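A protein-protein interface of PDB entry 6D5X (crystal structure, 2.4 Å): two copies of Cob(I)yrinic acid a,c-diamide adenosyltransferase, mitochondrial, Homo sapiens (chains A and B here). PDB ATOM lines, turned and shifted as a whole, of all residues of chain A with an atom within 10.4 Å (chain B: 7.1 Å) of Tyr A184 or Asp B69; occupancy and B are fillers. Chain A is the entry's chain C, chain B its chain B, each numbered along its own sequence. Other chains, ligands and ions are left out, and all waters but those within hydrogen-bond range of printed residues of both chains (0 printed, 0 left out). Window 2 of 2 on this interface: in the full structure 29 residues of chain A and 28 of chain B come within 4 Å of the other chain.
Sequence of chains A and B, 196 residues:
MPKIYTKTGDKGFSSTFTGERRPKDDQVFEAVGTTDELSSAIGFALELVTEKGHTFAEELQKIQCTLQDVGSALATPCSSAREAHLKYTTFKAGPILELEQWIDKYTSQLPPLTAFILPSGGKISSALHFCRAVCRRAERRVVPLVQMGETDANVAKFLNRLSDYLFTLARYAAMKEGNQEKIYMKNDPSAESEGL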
ATOM      1  N   LEU A 113      -4.990  30.066 -13.746  1.00  0.00           N
ATOM      2  CA  LEU A 113      -3.700  29.456 -14.038  1.00  0.00           C
ATOM      3  C   LEU A 113      -3.848  28.499 -15.211  1.00  0.00           C
ATOM      4  O   LEU A 113      -4.699  27.604 -15.192  1.00  0.00           O
ATOM      5  CB  LEU A 113      -3.154  28.714 -12.816  1.00  0.00           C
ATOM      6  CG  LEU A 113      -1.734  28.168 -12.969  1.00  0.00           C
ATOM      7  CD1 LEU A 113      -0.837  29.206 -13.635  1.00  0.00           C
ATOM      8  CD2 LEU A 113      -1.172  27.761 -11.617  1.00  0.00           C
ATOM      9  N   THR A 114      -3.021  28.710 -16.232  1.00  0.00           N
ATOM     10  CA  THR A 114      -3.125  28.000 -17.496  1.00  0.00           C
ATOM     11  C   THR A 114      -1.942  27.099 -17.817  1.00  0.00           C
ATOM     12  O   THR A 114      -2.125  26.105 -18.522  1.00  0.00           O
ATOM     13  CB  THR A 114      -3.306  29.008 -18.644  1.00  0.00           C
ATOM     14  OG1 THR A 114      -3.017  28.375 -19.896  1.00  0.00           O
ATOM     15  CG2 THR A 114      -2.387  30.218 -18.454  1.00  0.00           C
ATOM     16  N   ALA A 115      -0.740  27.415 -17.339  1.00  0.00           N
ATOM     17  CA  ALA A 115       0.452  26.667 -17.714  1.00  0.00           C
ATOM     18  C   ALA A 115       1.227  26.264 -16.466  1.00  0.00           C
ATOM     19  O   ALA A 115       0.881  26.631 -15.339  1.00  0.00           O
ATOM     20  CB  ALA A 115       1.340  27.483 -18.662  1.00  0.00           C
ATOM     21  N   PHE A 116       2.293  25.498 -16.683  1.00  0.00           N
ATOM     22  CA  PHE A 116       3.150  25.060 -15.594  1.00  0.00           C
ATOM     23  C   PHE A 116       4.045  26.204 -15.133  1.00  0.00           C
ATOM     24  O   PHE A 116       4.563  26.974 -15.948  1.00  0.00           O
ATOM     25  CB  PHE A 116       3.997  23.868 -16.038  1.00  0.00           C
ATOM     26  CG  PHE A 116       3.259  22.561 -16.018  1.00  0.00           C
ATOM     27  CD1 PHE A 116       2.948  21.911 -17.201  1.00  0.00           C
ATOM     28  CD2 PHE A 116       2.866  21.987 -14.820  1.00  0.00           C
ATOM     29  CE1 PHE A 116       2.269  20.706 -17.191  1.00  0.00           C
ATOM     30  CE2 PHE A 116       2.185  20.782 -14.803  1.00  0.00           C
ATOM     31  CZ  PHE A 116       1.886  20.141 -15.991  1.00  0.00           C
ATOM     32  N   ILE A 117       4.237  26.306 -13.824  1.00  0.00           N
ATOM     33  CA  ILE A 117       5.024  27.370 -13.217  1.00  0.00           C
ATOM     34  C   ILE A 117       6.340  26.787 -12.720  1.00  0.00           C
ATOM     35  O   ILE A 117       6.356  25.728 -12.083  1.00  0.00           O
ATOM     36  CB  ILE A 117       4.245  28.046 -12.076  1.00  0.00           C
ATOM     37  CG1 ILE A 117       3.167  28.964 -12.644  1.00  0.00           C
ATOM     38  CG2 ILE A 117       5.164  28.839 -11.178  1.00  0.00           C
ATOM     39  CD1 ILE A 117       2.267  29.527 -11.587  1.00  0.00           C
ATOM     40  N   LEU A 118       7.448  27.481 -13.017  1.00  0.00           N
ATOM     41  CA  LEU A 118       8.738  27.170 -12.420  1.00  0.00           C
ATOM     42  C   LEU A 118       8.887  27.871 -11.074  1.00  0.00           C
ATOM     43  O   LEU A 118       8.368  28.976 -10.884  1.00  0.00           O
ATOM     44  CB  LEU A 118       9.879  27.595 -13.339  1.00  0.00           C
ATOM     45  CG  LEU A 118       9.969  26.961 -14.726  1.00  0.00           C
ATOM     46  CD1 LEU A 118      11.149  27.544 -15.505  1.00  0.00           C
ATOM     47  CD2 LEU A 118      10.067  25.449 -14.617  1.00  0.00           C
ATOM     48  N   PRO A 119       9.565  27.249 -10.112  1.00  0.00           N
ATOM     49  CA  PRO A 119       9.828  27.938  -8.838  1.00  0.00           C
ATOM     50  C   PRO A 119      10.542  29.260  -9.081  1.00  0.00           C
ATOM     51  O   PRO A 119      11.666  29.296  -9.589  1.00  0.00           O
ATOM     52  CB  PRO A 119      10.709  26.942  -8.075  1.00  0.00           C
ATOM     53  CG  PRO A 119      10.368  25.596  -8.677  1.00  0.00           C
ATOM     54  CD  PRO A 119      10.100  25.875 -10.128  1.00  0.00           C
ATOM     55  N   SER A 120       9.874  30.355  -8.715  1.00  0.00           N
ATOM     56  CA  SER A 120      10.338  31.698  -9.045  1.00  0.00           C
ATOM     57  C   SER A 120       9.423  32.743  -8.422  1.00  0.00           C
ATOM     58  O   SER A 120       8.593  32.415  -7.568  1.00  0.00           O
ATOM     59  CB  SER A 120      10.384  31.894 -10.563  1.00  0.00           C
ATOM     60  OG  SER A 120       9.151  31.523 -11.162  1.00  0.00           O
ATOM     61  N   GLN A 180       6.580  38.519 -12.125  1.00  0.00           N
ATOM     62  CA  GLN A 180       5.975  37.494 -12.959  1.00  0.00           C
ATOM     63  C   GLN A 180       6.788  36.219 -12.794  1.00  0.00           C
ATOM     64  O   GLN A 180       8.021  36.248 -12.882  1.00  0.00           O
ATOM     65  CB  GLN A 180       5.932  37.922 -14.427  1.00  0.00           C
ATOM     66  CG  GLN A 180       5.076  37.022 -15.307  1.00  0.00           C
ATOM     67  CD  GLN A 180       4.927  37.543 -16.723  1.00  0.00           C
ATOM     68  OE1 GLN A 180       5.198  38.712 -17.003  1.00  0.00           O
ATOM     69  NE2 GLN A 180       4.494  36.672 -17.630  1.00  0.00           N
ATOM     70  N   GLU A 181       6.100  35.108 -12.556  1.00  0.00           N
ATOM     71  CA  GLU A 181       6.802  33.845 -12.423  1.00  0.00           C
ATOM     72  C   GLU A 181       7.288  33.387 -13.792  1.00  0.00           C
ATOM     73  O   GLU A 181       6.811  33.836 -14.838  1.00  0.00           O
ATOM     74  CB  GLU A 181       5.896  32.772 -11.815  1.00  0.00           C
ATOM     75  CG  GLU A 181       5.192  33.188 -10.544  1.00  0.00           C
ATOM     76  CD  GLU A 181       3.805  33.719 -10.816  1.00  0.00           C
ATOM     77  OE1 GLU A 181       3.592  34.301 -11.902  1.00  0.00           O
ATOM     78  OE2 GLU A 181       2.923  33.547  -9.950  1.00  0.00           O
ATOM     79  N   LYS A 182       8.255  32.483 -13.772  1.00  0.00           N
ATOM     80  CA  LYS A 182       8.793  31.938 -15.003  1.00  0.00           C
ATOM     81  C   LYS A 182       7.981  30.703 -15.344  1.00  0.00           C
ATOM     82  O   LYS A 182       7.479  29.998 -14.463  1.00  0.00           O
ATOM     83  CB  LYS A 182      10.283  31.597 -14.865  1.00  0.00           C
ATOM     84  CG  LYS A 182      11.190  32.810 -14.650  1.00  0.00           C
ATOM     85  CD  LYS A 182      11.007  33.835 -15.763  1.00  0.00           C
ATOM     86  CE  LYS A 182      12.141  34.853 -15.803  1.00  0.00           C
ATOM     87  NZ  LYS A 182      12.236  35.653 -14.551  1.00  0.00           N
ATOM     88  N   ILE A 183       7.850  30.446 -16.635  1.00  0.00           N
ATOM     89  CA  ILE A 183       6.884  29.484 -17.145  1.00  0.00           C
ATOM     90  C   ILE A 183       7.626  28.388 -17.886  1.00  0.00           C
ATOM     91  O   ILE A 183       8.628  28.648 -18.560  1.00  0.00           O
ATOM     92  CB  ILE A 183       5.857  30.174 -18.068  1.00  0.00           C
ATOM     93  CG1 ILE A 183       4.896  29.153 -18.672  1.00  0.00           C
ATOM     94  CG2 ILE A 183       6.559  30.958 -19.171  1.00  0.00           C
ATOM     95  CD1 ILE A 183       3.923  29.748 -19.659  1.00  0.00           C
ATOM     96  N   TYR A 184       7.159  27.155 -17.719  1.00  0.00           N
ATOM     97  CA  TYR A 184       7.880  26.032 -18.284  1.00  0.00           C
ATOM     98  C   TYR A 184       7.844  26.140 -19.801  1.00  0.00           C
ATOM     99  O   TYR A 184       6.854  26.587 -20.386  1.00  0.00           O
ATOM    100  CB  TYR A 184       7.268  24.713 -17.811  1.00  0.00           C
ATOM    101  CG  TYR A 184       7.686  23.529 -18.643  1.00  0.00           C
ATOM    102  CD1 TYR A 184       6.841  23.009 -19.616  1.00  0.00           C
ATOM    103  CD2 TYR A 184       8.932  22.940 -18.471  1.00  0.00           C
ATOM    104  CE1 TYR A 184       7.220  21.932 -20.389  1.00  0.00           C
ATOM    105  CE2 TYR A 184       9.319  21.859 -19.237  1.00  0.00           C
ATOM    106  CZ  TYR A 184       8.457  21.360 -20.193  1.00  0.00           C
ATOM    107  OH  TYR A 184       8.838  20.285 -20.959  1.00  0.00           O
ATOM    108  N   MET A 185       8.930  25.729 -20.443  1.00  0.00           N
ATOM    109  CA  MET A 185       8.993  25.728 -21.897  1.00  0.00           C
ATOM    110  C   MET A 185       9.770  24.506 -22.353  1.00  0.00           C
ATOM    111  O   MET A 185      10.851  24.224 -21.828  1.00  0.00           O
ATOM    112  CB  MET A 185       9.639  27.015 -22.421  1.00  0.00           C
ATOM    113  CG  MET A 185      10.842  27.465 -21.612  1.00  0.00           C
ATOM    114  SD  MET A 185      11.505  29.057 -22.138  1.00  0.00           S
ATOM    115  CE  MET A 185      10.158  30.159 -21.710  1.00  0.00           C
ATOM    116  N   LYS A 186       9.211  23.785 -23.323  1.00  0.00           N
ATOM    117  CA  LYS A 186       9.826  22.556 -23.802  1.00  0.00           C
ATOM    118  C   LYS A 186      11.158  22.844 -24.484  1.00  0.00           C
ATOM    119  O   LYS A 186      11.381  23.929 -25.029  1.00  0.00           O
ATOM    120  CB  LYS A 186       8.902  21.841 -24.787  1.00  0.00           C
ATOM    121  CG  LYS A 186       7.422  22.071 -24.543  1.00  0.00           C
ATOM    122  CD  LYS A 186       6.586  21.498 -25.675  1.00  0.00           C
ATOM    123  CE  LYS A 186       5.118  21.844 -25.500  1.00  0.00           C
ATOM    124  NZ  LYS A 186       4.914  23.316 -25.388  1.00  0.00           N
ATOM    125  N   ASN A 187      12.041  21.849 -24.454  1.00  0.00           N
ATOM    126  CA  ASN A 187      13.308  21.891 -25.181  1.00  0.00           C
ATOM    127  C   ASN A 187      14.126  23.149 -24.889  1.00  0.00           C
ATOM    128  O   ASN A 187      14.738  23.272 -23.828  1.00  0.00           O
ATOM    129  CB  ASN A 187      13.044  21.772 -26.685  1.00  0.00           C
ATOM    130  CG  ASN A 187      14.216  22.236 -27.520  1.00  0.00           C
ATOM    131  OD1 ASN A 187      15.252  21.574 -27.580  1.00  0.00           O
ATOM    132  ND2 ASN A 187      14.056  23.376 -28.182  1.00  0.00           N
ATOM    133  N   THR B  35      13.465  15.661  -7.070  1.00  0.00           N
ATOM    134  CA  THR B  35      13.742  16.504  -8.229  1.00  0.00           C
ATOM    135  C   THR B  35      13.045  17.855  -8.094  1.00  0.00           C
ATOM    136  O   THR B  35      13.622  18.909  -8.414  1.00  0.00           O
ATOM    137  CB  THR B  35      13.286  15.795  -9.504  1.00  0.00           C
ATOM    138  OG1 THR B  35      14.027  14.579  -9.666  1.00  0.00           O
ATOM    139  CG2 THR B  35      13.501  16.686 -10.718  1.00  0.00           C
ATOM    140  N   LYS B  62      17.007  27.215 -17.706  1.00  0.00           N
ATOM    141  CA  LYS B  62      16.932  26.088 -18.632  1.00  0.00           C
ATOM    142  C   LYS B  62      16.993  24.763 -17.880  1.00  0.00           C
ATOM    143  O   LYS B  62      16.249  23.818 -18.186  1.00  0.00           O
ATOM    144  CB  LYS B  62      18.078  26.169 -19.639  1.00  0.00           C
ATOM    145  CG  LYS B  62      17.960  27.296 -20.651  1.00  0.00           C
ATOM    146  CD  LYS B  62      19.189  27.345 -21.557  1.00  0.00           C
ATOM    147  CE  LYS B  62      19.116  28.496 -22.554  1.00  0.00           C
ATOM    148  NZ  LYS B  62      20.346  28.574 -23.393  1.00  0.00           N
ATOM    149  N   ILE B  63      17.884  24.681 -16.894  1.00  0.00           N
ATOM    150  CA  ILE B  63      18.013  23.473 -16.086  1.00  0.00           C
ATOM    151  C   ILE B  63      16.720  23.182 -15.332  1.00  0.00           C
ATOM    152  O   ILE B  63      16.331  22.021 -15.172  1.00  0.00           O
ATOM    153  CB  ILE B  63      19.221  23.593 -15.144  1.00  0.00           C
ATOM    154  CG1 ILE B  63      20.520  23.455 -15.947  1.00  0.00           C
ATOM    155  CG2 ILE B  63      19.140  22.554 -14.044  1.00  0.00           C
ATOM    156  CD1 ILE B  63      21.738  24.069 -15.285  1.00  0.00           C
ATOM    157  N   GLN B  64      16.048  24.223 -14.830  1.00  0.00           N
ATOM    158  CA  GLN B  64      14.765  24.006 -14.162  1.00  0.00           C
ATOM    159  C   GLN B  64      13.743  23.380 -15.109  1.00  0.00           C
ATOM    160  O   GLN B  64      13.004  22.456 -14.729  1.00  0.00           O
ATOM    161  CB  GLN B  64      14.230  25.319 -13.592  1.00  0.00           C
ATOM    162  CG  GLN B  64      14.984  25.814 -12.377  1.00  0.00           C
ATOM    163  CD  GLN B  64      14.343  27.047 -11.771  1.00  0.00           C
ATOM    164  OE1 GLN B  64      14.304  28.106 -12.397  1.00  0.00           O
ATOM    165  NE2 GLN B  64      13.842  26.919 -10.546  1.00  0.00           N
ATOM    166  N   CYS B  65      13.685  23.869 -16.349  1.00  0.00           N
ATOM    167  CA  CYS B  65      12.787  23.245 -17.326  1.00  0.00           C
ATOM    168  C   CYS B  65      13.147  21.775 -17.545  1.00  0.00           C
ATOM    169  O   CYS B  65      12.271  20.889 -17.578  1.00  0.00           O
ATOM    170  CB  CYS B  65      12.831  24.014 -18.646  1.00  0.00           C
ATOM    171  SG  CYS B  65      12.099  25.663 -18.566  1.00  0.00           S
ATOM    172  N   THR B  66      14.442  21.495 -17.703  1.00  0.00           N
ATOM    173  CA  THR B  66      14.876  20.109 -17.858  1.00  0.00           C
ATOM    174  C   THR B  66      14.486  19.268 -16.644  1.00  0.00           C
ATOM    175  O   THR B  66      14.179  18.079 -16.781  1.00  0.00           O
ATOM    176  CB  THR B  66      16.382  20.043 -18.100  1.00  0.00           C
ATOM    177  OG1 THR B  66      16.701  20.746 -19.306  1.00  0.00           O
ATOM    178  CG2 THR B  66      16.835  18.596 -18.249  1.00  0.00           C
ATOM    179  N   LEU B  67      14.504  19.863 -15.450  1.00  0.00           N
ATOM    180  CA  LEU B  67      14.112  19.119 -14.256  1.00  0.00           C
ATOM    181  C   LEU B  67      12.625  18.799 -14.264  1.00  0.00           C
ATOM    182  O   LEU B  67      12.214  17.747 -13.761  1.00  0.00           O
ATOM    183  CB  LEU B  67      14.487  19.893 -12.990  1.00  0.00           C
ATOM    184  CG  LEU B  67      15.993  19.972 -12.706  1.00  0.00           C
ATOM    185  CD1 LEU B  67      16.269  20.735 -11.421  1.00  0.00           C
ATOM    186  CD2 LEU B  67      16.623  18.592 -12.644  1.00  0.00           C
ATOM    187  N   GLN B  68      11.810  19.680 -14.844  1.00  0.00           N
ATOM    188  CA  GLN B  68      10.412  19.319 -15.064  1.00  0.00           C
ATOM    189  C   GLN B  68      10.303  18.111 -15.991  1.00  0.00           C
ATOM    190  O   GLN B  68       9.521  17.179 -15.737  1.00  0.00           O
ATOM    191  CB  GLN B  68       9.650  20.510 -15.648  1.00  0.00           C
ATOM    192  CG  GLN B  68       8.250  20.182 -16.126  1.00  0.00           C
ATOM    193  CD  GLN B  68       7.173  20.770 -15.249  1.00  0.00           C
ATOM    194  OE1 GLN B  68       7.416  21.118 -14.095  1.00  0.00           O
ATOM    195  NE2 GLN B  68       5.970  20.889 -15.796  1.00  0.00           N
ATOM    196  N   ASP B  69      11.127  18.081 -17.040  1.00  0.00           N
ATOM    197  CA  ASP B  69      11.116  16.921 -17.935  1.00  0.00           C
ATOM    198  C   ASP B  69      11.577  15.655 -17.215  1.00  0.00           C
ATOM    199  O   ASP B  69      11.039  14.563 -17.447  1.00  0.00           O
ATOM    200  CB  ASP B  69      11.981  17.191 -19.166  1.00  0.00           C
ATOM    201  CG  ASP B  69      11.388  18.257 -20.066  1.00  0.00           C
ATOM    202  OD1 ASP B  69      12.160  18.938 -20.774  1.00  0.00           O
ATOM    203  OD2 ASP B  69      10.153  18.439 -20.037  1.00  0.00           O
ATOM    204  N   VAL B  70      12.566  15.785 -16.329  1.00  0.00           N
ATOM    205  CA  VAL B  70      13.081  14.638 -15.584  1.00  0.00           C
ATOM    206  C   VAL B  70      12.023  14.109 -14.627  1.00  0.00           C
ATOM    207  O   VAL B  70      11.857  12.892 -14.468  1.00  0.00           O
ATOM    208  CB  VAL B  70      14.366  15.032 -14.829  1.00  0.00           C
ATOM    209  CG1 VAL B  70      14.742  13.978 -13.801  1.00  0.00           C
ATOM    210  CG2 VAL B  70      15.510  15.250 -15.791  1.00  0.00           C
ATOM    211  N   GLY B  71      11.277  15.015 -13.990  1.00  0.00           N
ATOM    212  CA  GLY B  71      10.164  14.595 -13.156  1.00  0.00           C
ATOM    213  C   GLY B  71       9.102  13.855 -13.944  1.00  0.00           C
ATOM    214  O   GLY B  71       8.554  12.853 -13.478  1.00  0.00           O
ATOM    215  N   SER B  72       8.803  14.334 -15.156  1.00  0.00           N
ATOM    216  CA  SER B  72       7.837  13.629 -15.990  1.00  0.00           C
ATOM    217  C   SER B  72       8.333  12.236 -16.356  1.00  0.00           C
ATOM    218  O   SER B  72       7.562  11.270 -16.329  1.00  0.00           O
ATOM    219  CB  SER B  72       7.531  14.437 -17.252  1.00  0.00           C
ATOM    220  OG  SER B  72       6.721  15.559 -16.952  1.00  0.00           O
ATOM    221  N   ALA B  73       9.621  12.107 -16.682  1.00  0.00           N
ATOM    222  CA  ALA B  73      10.171  10.794 -17.014  1.00  0.00           C
ATOM    223  C   ALA B  73      10.090   9.841 -15.825  1.00  0.00           C
ATOM    224  O   ALA B  73       9.669   8.685 -15.968  1.00  0.00           O
ATOM    225  CB  ALA B  73      11.613  10.931 -17.502  1.00  0.00           C
ATOM    226  N   LEU B  74      10.493  10.308 -14.640  1.00  0.00           N
ATOM    227  CA  LEU B  74      10.473   9.452 -13.456  1.00  0.00           C
ATOM    228  C   LEU B  74       9.062   9.000 -13.101  1.00  0.00           C
ATOM    229  O   LEU B  74       8.888   7.954 -12.467  1.00  0.00           O
ATOM    230  CB  LEU B  74      11.106  10.178 -12.267  1.00  0.00           C
ATOM    231  CG  LEU B  74      12.588  10.549 -12.388  1.00  0.00           C
ATOM    232  CD1 LEU B  74      13.015  11.475 -11.255  1.00  0.00           C
ATOM    233  CD2 LEU B  74      13.464   9.302 -12.424  1.00  0.00           C
ATOM    234  N   ALA B  75       8.049   9.778 -13.477  1.00  0.00           N
ATOM    235  CA  ALA B  75       6.663   9.453 -13.160  1.00  0.00           C
ATOM    236  C   ALA B  75       6.050   8.420 -14.099  1.00  0.00           C
ATOM    237  O   ALA B  75       4.914   7.995 -13.866  1.00  0.00           O
ATOM    238  CB  ALA B  75       5.812  10.725 -13.167  1.00  0.00           C
ATOM    239  N   PHE B  91      14.626   9.433 -22.467  1.00  0.00           N
ATOM    240  CA  PHE B  91      15.211  10.701 -22.058  1.00  0.00           C
ATOM    241  C   PHE B  91      16.452  10.963 -22.900  1.00  0.00           C
ATOM    242  O   PHE B  91      17.440  10.224 -22.812  1.00  0.00           O
ATOM    243  CB  PHE B  91      15.570  10.688 -20.575  1.00  0.00           C
ATOM    244  CG  PHE B  91      15.940  12.039 -20.039  1.00  0.00           C
ATOM    245  CD1 PHE B  91      14.958  12.934 -19.650  1.00  0.00           C
ATOM    246  CD2 PHE B  91      17.267  12.424 -19.947  1.00  0.00           C
ATOM    247  CE1 PHE B  91      15.293  14.184 -19.167  1.00  0.00           C
ATOM    248  CE2 PHE B  91      17.611  13.674 -19.462  1.00  0.00           C
ATOM    249  CZ  PHE B  91      16.622  14.554 -19.073  1.00  0.00           C
ATOM    250  N   PRO B  95      20.572  17.594 -23.198  1.00  0.00           N
ATOM    251  CA  PRO B  95      20.896  18.387 -21.996  1.00  0.00           C
ATOM    252  C   PRO B  95      22.206  17.997 -21.331  1.00  0.00           C
ATOM    253  O   PRO B  95      22.917  18.877 -20.826  1.00  0.00           O
ATOM    254  CB  PRO B  95      19.694  18.125 -21.074  1.00  0.00           C
ATOM    255  CG  PRO B  95      18.585  17.786 -21.999  1.00  0.00           C
ATOM    256  CD  PRO B  95      19.211  17.033 -23.134  1.00  0.00           C
ATOM    257  N   VAL B 155      18.707   9.696 -17.287  1.00  0.00           N
ATOM    258  CA  VAL B 155      18.201  10.566 -16.228  1.00  0.00           C
ATOM    259  C   VAL B 155      19.225  10.680 -15.101  1.00  0.00           C
ATOM    260  O   VAL B 155      19.564  11.782 -14.633  1.00  0.00           O
ATOM    261  CB  VAL B 155      16.852  10.031 -15.706  1.00  0.00           C
ATOM    262  CG1 VAL B 155      16.378  10.848 -14.530  1.00  0.00           C
ATOM    263  CG2 VAL B 155      15.806  10.005 -16.818  1.00  0.00           C
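Gln B68 touches Phe A116.
Cys B65 touches Leu A118.
Tyr A184 touches Cys B65.
CG of Gln B68 touches CD2 of Tyr A184, 3.7 Å away.
The backbone carbonyl oxygen (O) of Gln B68 lies within hydrogen-bond range of the side-chain hydroxyl (OG) of Ser B72.
The backbone NH (N) of Tyr A184 lies within hydrogen-bond range of the backbone carbonyl oxygen (O) of Phe A116, 3.1 Å away.
O of Leu A118 lies within hydrogen-bond range of OG of Ser A120.
N of Leu A118 is in hydrogen-bond range of O of Lys A182 (2.9 Å).
Of the 18 printed residues of chain B, 4 touch a printed residue of chain A.
Printed residues of chain B that touch a printed residue of chain A: Gln B64, Cys B65, Gln B68 and Asp B69.
Along chain A the printed residues that touch a printed residue of chain B span positions 116 to 185.
Among the printed residues, no Asp or Glu carboxylate lies within 4 Å of a Lys or Arg side-chain nitrogen of the other chain.
The side-chain amide nitrogen (NE2) of Gln B64 sits at hydrogen-bond distance from the backbone carbonyl oxygen (O) of Pro A119.
SG of Cys B65 lies within hydrogen-bond range of N of Met A185.
The side-chain carboxylate (OD2) of Asp B69 lies within hydrogen-bond range of the side-chain hydroxyl (OH) of Tyr A184 (2.4 Å).
No position is printed for both chains.
Of the 7 pairs that touch across the chains among the printed residues, none has its exchanged pair printed and touching as well.
Tyr A184 touches just these residues of chain B: Cys B65 (3.5 Å), Gln B68 (3.7 Å) and Asp B69 (2.4 Å).
Of the printed residues of chain A, Asp B69 touches Tyr A184 (2.4 Å).
Of the printed residues of chain A, Cys B65 touches Leu A118 (3.7 Å), Tyr A184 (3.5 Å) and Met A185 (3.7 Å).
No residue of chain A comes within 4 Å of Thr B66.
No residue of chain A comes within 4 Å of Val B70.
No residue of chain A comes within 4 Å of Gly B71.
No residue of chain A comes within 4 Å of Ser B72.
Ala B73 touches none of the printed residues of chain A.
Of the printed residues of chain B, Met A185 touches Cys B65 (3.7 Å).
Printed residues of chain B within 4 Å of Phe A116: Gln B68.
Ala B75 touches none of the printed residues of chain A.
The nearest residue of chain B that does not touch Tyr A184 is Thr B66 (5.4 Å).
The nearest printed residue of chain A that does not touch Gln B64 is Leu A118 (4.2 Å).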
